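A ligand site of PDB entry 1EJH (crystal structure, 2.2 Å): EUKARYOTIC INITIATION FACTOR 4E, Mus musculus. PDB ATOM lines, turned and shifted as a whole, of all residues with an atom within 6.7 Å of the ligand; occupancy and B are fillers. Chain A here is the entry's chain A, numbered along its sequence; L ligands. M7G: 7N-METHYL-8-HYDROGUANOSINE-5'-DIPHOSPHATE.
The backbone NH (N) of Trp 75 lies within hydrogen-bond range of an oxygen (O6) of the ligand (2.6 Å). O1B of the ligand is in salt-bridge range of NE of Arg 130, at 2.7 Å. OE2 of Glu 76 sits at hydrogen-bond distance from N2 of the ligand (2.9 Å). NZ of Lys 135 is in salt-bridge range of O2B of the ligand, 3.1 Å away.
The guanidinium group (NH2) of Arg 130 sits close to the side-chain amide nitrogen (ND2) of Asn 128 (3.4 Å). NH2 of Arg 130 is in salt-bridge range of OD1 of Asp 63, 2.6 Å away. O of Lys 135 is in hydrogen-bond range of N of Asn 128 (2.8 Å). The side-chain amide oxygen (OE1) of Gln 30 sits close to the side-chain sulfur (SD) of Met 74 (3.2 Å).
Trp 29 touches the ligand (CD1 to O4', 3.5 Å). CA of Met 74 touches O6 of the ligand (3.1 Å). CH2 of Trp 139 touches O6 of the ligand, 3.9 Å away. Within 4 Å of the ligand: Trp 29, Met 74, Trp 75, Glu 76, Arg 130, Lys 135 and Trp 139. The nearest printed residue that does not touch the ligand is Asn 128 (4.2 Å).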
ATOM      1  N   PHE A  21       8.828  30.372  18.944  1.00  0.00           N
ATOM      2  CA  PHE A  21       8.772  31.183  17.738  1.00  0.00           C
ATOM      3  C   PHE A  21       7.580  30.716  16.934  1.00  0.00           C
ATOM      4  O   PHE A  21       7.384  29.510  16.727  1.00  0.00           O
ATOM      5  CB  PHE A  21      10.033  31.006  16.897  1.00  0.00           C
ATOM      6  CG  PHE A  21       9.979  31.751  15.594  1.00  0.00           C
ATOM      7  CD1 PHE A  21      10.241  33.114  15.539  1.00  0.00           C
ATOM      8  CD2 PHE A  21       9.639  31.093  14.417  1.00  0.00           C
ATOM      9  CE1 PHE A  21      10.175  33.810  14.332  1.00  0.00           C
ATOM     10  CE2 PHE A  21       9.572  31.777  13.202  1.00  0.00           C
ATOM     11  CZ  PHE A  21       9.832  33.142  13.156  1.00  0.00           C
ATOM     12  N   ASN A  23       5.875  31.125  13.266  1.00  0.00           N
ATOM     13  CA  ASN A  23       6.160  31.664  11.951  1.00  0.00           C
ATOM     14  C   ASN A  23       4.958  32.382  11.352  1.00  0.00           C
ATOM     15  O   ASN A  23       4.359  31.933  10.364  1.00  0.00           O
ATOM     16  CB  ASN A  23       6.644  30.578  10.982  1.00  0.00           C
ATOM     17  CG  ASN A  23       7.363  31.166   9.777  1.00  0.00           C
ATOM     18  OD1 ASN A  23       7.771  30.439   8.869  1.00  0.00           O
ATOM     19  ND2 ASN A  23       7.539  32.480   9.765  1.00  0.00           N
ATOM     20  N   TRP A  29      11.842  38.266  11.958  1.00  0.00           N
ATOM     21  CA  TRP A  29      12.118  36.987  12.577  1.00  0.00           C
ATOM     22  C   TRP A  29      12.206  37.197  14.079  1.00  0.00           C
ATOM     23  O   TRP A  29      11.530  36.511  14.856  1.00  0.00           O
ATOM     24  CB  TRP A  29      13.449  36.420  12.058  1.00  0.00           C
ATOM     25  CG  TRP A  29      13.780  35.085  12.647  1.00  0.00           C
ATOM     26  CD1 TRP A  29      13.342  33.862  12.213  1.00  0.00           C
ATOM     27  CD2 TRP A  29      14.577  34.834  13.807  1.00  0.00           C
ATOM     28  NE1 TRP A  29      13.819  32.868  13.045  1.00  0.00           N
ATOM     29  CE2 TRP A  29      14.581  33.444  14.021  1.00  0.00           C
ATOM     30  CE3 TRP A  29      15.290  35.663  14.689  1.00  0.00           C
ATOM     31  CZ2 TRP A  29      15.265  32.855  15.088  1.00  0.00           C
ATOM     32  CZ3 TRP A  29      15.968  35.083  15.742  1.00  0.00           C
ATOM     33  CH2 TRP A  29      15.953  33.683  15.935  1.00  0.00           C
ATOM     34  N   GLN A  30      13.022  38.154  14.481  1.00  0.00           N
ATOM     35  CA  GLN A  30      13.218  38.489  15.881  1.00  0.00           C
ATOM     36  C   GLN A  30      11.966  39.106  16.492  1.00  0.00           C
ATOM     37  O   GLN A  30      12.066  39.877  17.449  1.00  0.00           O
ATOM     38  CB  GLN A  30      14.363  39.493  15.993  1.00  0.00           C
ATOM     39  CG  GLN A  30      14.899  39.589  17.379  1.00  0.00           C
ATOM     40  CD  GLN A  30      16.214  40.310  17.423  1.00  0.00           C
ATOM     41  OE1 GLN A  30      17.024  40.202  16.500  1.00  0.00           O
ATOM     42  NE2 GLN A  30      16.456  41.014  18.522  1.00  0.00           N
ATOM     43  N   GLY A  61       7.015  25.524  10.855  1.00  0.00           N
ATOM     44  CA  GLY A  61       7.545  26.869  10.957  1.00  0.00           C
ATOM     45  C   GLY A  61       7.760  27.404  12.370  1.00  0.00           C
ATOM     46  O   GLY A  61       8.204  28.524  12.541  1.00  0.00           O
ATOM     47  N   ASP A  63       9.370  27.085  16.449  1.00  0.00           N
ATOM     48  CA  ASP A  63      10.515  26.576  17.183  1.00  0.00           C
ATOM     49  C   ASP A  63      10.347  26.768  18.675  1.00  0.00           C
ATOM     50  O   ASP A  63       9.616  27.653  19.110  1.00  0.00           O
ATOM     51  CB  ASP A  63      11.818  27.300  16.838  1.00  0.00           C
ATOM     52  CG  ASP A  63      11.916  27.724  15.413  1.00  0.00           C
ATOM     53  OD1 ASP A  63      11.643  26.901  14.508  1.00  0.00           O
ATOM     54  OD2 ASP A  63      12.299  28.907  15.204  1.00  0.00           O
ATOM     55  N   PRO A  73      17.942  33.489  22.081  1.00  0.00           N
ATOM     56  CA  PRO A  73      18.082  32.413  21.103  1.00  0.00           C
ATOM     57  C   PRO A  73      18.342  32.895  19.684  1.00  0.00           C
ATOM     58  O   PRO A  73      17.569  32.574  18.785  1.00  0.00           O
ATOM     59  CB  PRO A  73      16.748  31.684  21.236  1.00  0.00           C
ATOM     60  CG  PRO A  73      15.796  32.809  21.472  1.00  0.00           C
ATOM     61  CD  PRO A  73      16.541  33.667  22.485  1.00  0.00           C
ATOM     62  N   MET A  74      19.420  33.647  19.488  1.00  0.00           N
ATOM     63  CA  MET A  74      19.777  34.173  18.166  1.00  0.00           C
ATOM     64  C   MET A  74      21.297  34.191  17.946  1.00  0.00           C
ATOM     65  O   MET A  74      22.074  34.432  18.877  1.00  0.00           O
ATOM     66  CB  MET A  74      19.245  35.600  17.994  1.00  0.00           C
ATOM     67  CG  MET A  74      17.805  35.763  18.418  1.00  0.00           C
ATOM     68  SD  MET A  74      17.205  37.430  18.172  1.00  0.00           S
ATOM     69  CE  MET A  74      18.386  38.363  19.174  1.00  0.00           C
ATOM     70  N   TRP A  75      21.709  33.956  16.698  1.00  0.00           N
ATOM     71  CA  TRP A  75      23.112  33.936  16.335  1.00  0.00           C
ATOM     72  C   TRP A  75      23.826  35.185  16.844  1.00  0.00           C
ATOM     73  O   TRP A  75      24.858  35.104  17.510  1.00  0.00           O
ATOM     74  CB  TRP A  75      23.284  33.885  14.806  1.00  0.00           C
ATOM     75  CG  TRP A  75      22.683  32.678  14.115  1.00  0.00           C
ATOM     76  CD1 TRP A  75      22.551  31.407  14.623  1.00  0.00           C
ATOM     77  CD2 TRP A  75      22.157  32.622  12.782  1.00  0.00           C
ATOM     78  NE1 TRP A  75      21.976  30.576  13.688  1.00  0.00           N
ATOM     79  CE2 TRP A  75      21.723  31.291  12.543  1.00  0.00           C
ATOM     80  CE3 TRP A  75      22.005  33.566  11.747  1.00  0.00           C
ATOM     81  CZ2 TRP A  75      21.153  30.890  11.328  1.00  0.00           C
ATOM     82  CZ3 TRP A  75      21.434  33.167  10.541  1.00  0.00           C
ATOM     83  CH2 TRP A  75      21.021  31.829  10.349  1.00  0.00           C
ATOM     84  N   GLU A  76      23.261  36.332  16.522  1.00  0.00           N
ATOM     85  CA  GLU A  76      23.834  37.617  16.897  1.00  0.00           C
ATOM     86  C   GLU A  76      24.177  37.816  18.375  1.00  0.00           C
ATOM     87  O   GLU A  76      25.094  38.559  18.681  1.00  0.00           O
ATOM     88  CB  GLU A  76      22.925  38.757  16.445  1.00  0.00           C
ATOM     89  CG  GLU A  76      22.691  38.860  14.934  1.00  0.00           C
ATOM     90  CD  GLU A  76      21.707  37.807  14.398  1.00  0.00           C
ATOM     91  OE1 GLU A  76      21.097  37.076  15.207  1.00  0.00           O
ATOM     92  OE2 GLU A  76      21.556  37.731  13.165  1.00  0.00           O
ATOM     93  N   ARG A  85      26.578  25.144  16.613  1.00  0.00           N
ATOM     94  CA  ARG A  85      25.633  24.167  17.096  1.00  0.00           C
ATOM     95  C   ARG A  85      25.809  22.748  16.559  1.00  0.00           C
ATOM     96  O   ARG A  85      26.218  22.548  15.416  1.00  0.00           O
ATOM     97  CB  ARG A  85      24.209  24.644  16.739  1.00  0.00           C
ATOM     98  CG  ARG A  85      23.646  23.994  15.476  1.00  0.00           C
ATOM     99  CD  ARG A  85      23.428  24.953  14.323  1.00  0.00           C
ATOM    100  NE  ARG A  85      21.993  25.114  14.070  1.00  0.00           N
ATOM    101  CZ  ARG A  85      21.446  25.319  12.863  1.00  0.00           C
ATOM    102  NH1 ARG A  85      22.201  25.387  11.781  1.00  0.00           N
ATOM    103  NH2 ARG A  85      20.128  25.444  12.761  1.00  0.00           N
ATOM    104  N   VAL A 126      17.769  24.316  20.396  1.00  0.00           N
ATOM    105  CA  VAL A 126      16.657  24.747  19.552  1.00  0.00           C
ATOM    106  C   VAL A 126      16.022  23.572  18.815  1.00  0.00           C
ATOM    107  O   VAL A 126      16.731  22.682  18.326  1.00  0.00           O
ATOM    108  CB  VAL A 126      17.164  25.738  18.461  1.00  0.00           C
ATOM    109  CG1 VAL A 126      16.035  26.082  17.491  1.00  0.00           C
ATOM    110  CG2 VAL A 126      17.712  26.998  19.120  1.00  0.00           C
ATOM    111  N   ASN A 128      13.430  23.029  15.684  1.00  0.00           N
ATOM    112  CA  ASN A 128      12.665  23.665  14.614  1.00  0.00           C
ATOM    113  C   ASN A 128      11.735  22.604  14.015  1.00  0.00           C
ATOM    114  O   ASN A 128      12.174  21.517  13.656  1.00  0.00           O
ATOM    115  CB  ASN A 128      13.582  24.187  13.486  1.00  0.00           C
ATOM    116  CG  ASN A 128      14.705  25.056  13.976  1.00  0.00           C
ATOM    117  OD1 ASN A 128      15.892  24.712  13.826  1.00  0.00           O
ATOM    118  ND2 ASN A 128      14.366  26.212  14.550  1.00  0.00           N
ATOM    119  N   ARG A 130       9.576  21.801  10.910  1.00  0.00           N
ATOM    120  CA  ARG A 130       9.432  22.270   9.533  1.00  0.00           C
ATOM    121  C   ARG A 130       8.729  21.231   8.688  1.00  0.00           C
ATOM    122  O   ARG A 130       8.624  20.073   9.065  1.00  0.00           O
ATOM    123  CB  ARG A 130      10.815  22.565   8.916  1.00  0.00           C
ATOM    124  CG  ARG A 130      11.617  23.625   9.665  1.00  0.00           C
ATOM    125  CD  ARG A 130      11.073  25.015   9.407  1.00  0.00           C
ATOM    126  NE  ARG A 130      11.800  26.036  10.165  1.00  0.00           N
ATOM    127  CZ  ARG A 130      11.605  26.289  11.460  1.00  0.00           C
ATOM    128  NH1 ARG A 130      10.708  25.609  12.142  1.00  0.00           N
ATOM    129  NH2 ARG A 130      12.315  27.238  12.058  1.00  0.00           N
ATOM    130  N   GLY A 133      11.102  17.795   7.397  1.00  0.00           N
ATOM    131  CA  GLY A 133      11.962  17.251   8.435  1.00  0.00           C
ATOM    132  C   GLY A 133      12.183  18.273   9.540  1.00  0.00           C
ATOM    133  O   GLY A 133      12.200  19.476   9.285  1.00  0.00           O
ATOM    134  N   LYS A 135      14.412  19.645  13.089  1.00  0.00           N
ATOM    135  CA  LYS A 135      15.798  19.769  13.490  1.00  0.00           C
ATOM    136  C   LYS A 135      15.957  20.068  14.967  1.00  0.00           C
ATOM    137  O   LYS A 135      15.181  20.829  15.554  1.00  0.00           O
ATOM    138  CB  LYS A 135      16.469  20.891  12.689  1.00  0.00           C
ATOM    139  CG  LYS A 135      16.576  20.589  11.197  1.00  0.00           C
ATOM    140  CD  LYS A 135      17.145  21.780  10.417  1.00  0.00           C
ATOM    141  CE  LYS A 135      16.169  22.946  10.419  1.00  0.00           C
ATOM    142  NZ  LYS A 135      16.669  24.100   9.617  1.00  0.00           N
ATOM    143  N   TRP A 139      23.396  24.658  20.955  1.00  0.00           N
ATOM    144  CA  TRP A 139      24.290  25.776  20.647  1.00  0.00           C
ATOM    145  C   TRP A 139      25.351  25.912  21.751  1.00  0.00           C
ATOM    146  O   TRP A 139      25.050  25.708  22.912  1.00  0.00           O
ATOM    147  CB  TRP A 139      23.470  27.067  20.564  1.00  0.00           C
ATOM    148  CG  TRP A 139      22.474  27.151  19.432  1.00  0.00           C
ATOM    149  CD1 TRP A 139      21.817  26.121  18.831  1.00  0.00           C
ATOM    150  CD2 TRP A 139      22.010  28.346  18.798  1.00  0.00           C
ATOM    151  NE1 TRP A 139      20.969  26.600  17.854  1.00  0.00           N
ATOM    152  CE2 TRP A 139      21.070  27.962  17.808  1.00  0.00           C
ATOM    153  CE3 TRP A 139      22.296  29.710  18.976  1.00  0.00           C
ATOM    154  CZ2 TRP A 139      20.402  28.893  16.997  1.00  0.00           C
ATOM    155  CZ3 TRP A 139      21.639  30.638  18.167  1.00  0.00           C
ATOM    156  CH2 TRP A 139      20.699  30.224  17.185  1.00  0.00           C
ATOM    157  N   THR A 176      26.926  29.007   9.023  1.00  0.00           N
ATOM    158  CA  THR A 176      25.521  28.772   8.722  1.00  0.00           C
ATOM    159  C   THR A 176      24.910  30.075   8.217  1.00  0.00           C
ATOM    160  O   THR A 176      23.931  30.059   7.478  1.00  0.00           O
ATOM    161  CB  THR A 176      24.750  28.309   9.980  1.00  0.00           C
ATOM    162  OG1 THR A 176      25.239  27.036  10.398  1.00  0.00           O
ATOM    163  CG2 THR A 176      23.262  28.196   9.677  1.00  0.00           C
HETATM  164  PA  M7G L   1      15.817  28.334  10.480  1.00  0.00           P
HETATM  165  O1A M7G L   1      14.588  28.716  11.230  1.00  0.00           O
HETATM  166  O2A M7G L   1      16.943  28.201  11.435  1.00  0.00           O
HETATM  167  O3A M7G L   1      15.578  26.935   9.733  1.00  0.00           O
HETATM  168  O5' M7G L   1      16.180  29.483   9.369  1.00  0.00           O
HETATM  169  PB  M7G L   1      14.642  26.848   8.446  1.00  0.00           P
HETATM  170  O1B M7G L   1      13.420  27.669   8.672  1.00  0.00           O
HETATM  171  O2B M7G L   1      14.262  25.433   8.247  1.00  0.00           O
HETATM  172  O3B M7G L   1      15.374  27.353   7.275  1.00  0.00           O
HETATM  173  C5' M7G L   1      15.204  30.393   8.896  1.00  0.00           C
HETATM  174  C4' M7G L   1      15.657  31.801   8.688  1.00  0.00           C
HETATM  175  O4' M7G L   1      15.555  32.429   9.969  1.00  0.00           O
HETATM  176  C3' M7G L   1      17.113  32.010   8.366  1.00  0.00           C
HETATM  177  O3' M7G L   1      17.364  31.978   6.937  1.00  0.00           O
HETATM  178  C2' M7G L   1      17.357  33.484   8.833  1.00  0.00           C
HETATM  179  O2' M7G L   1      16.838  34.467   7.840  1.00  0.00           O
HETATM  180  C1' M7G L   1      16.557  33.458  10.138  1.00  0.00           C
HETATM  181  N9  M7G L   1      17.221  32.966  11.374  1.00  0.00           N
HETATM  182  C8  M7G L   1      17.363  31.739  11.940  1.00  0.00           C
HETATM  183  N7  M7G L   1      18.052  31.863  13.037  1.00  0.00           N
HETATM  184  CM7 M7G L   1      18.421  30.756  13.937  1.00  0.00           C
HETATM  185  C5  M7G L   1      18.442  33.289  13.307  1.00  0.00           C
HETATM  186  C6  M7G L   1      19.106  33.942  14.197  1.00  0.00           C
HETATM  187  O6  M7G L   1      19.629  33.379  15.203  1.00  0.00           O
HETATM  188  N1  M7G L   1      19.169  35.342  13.927  1.00  0.00           N
HETATM  189  C2  M7G L   1      18.598  35.975  12.833  1.00  0.00           C
HETATM  190  N2  M7G L   1      18.735  37.270  12.726  1.00  0.00           N
HETATM  191  N3  M7G L   1      17.905  35.287  11.886  1.00  0.00           N
HETATM  192  C4  M7G L   1      17.838  33.909  12.149  1.00  0.00           C
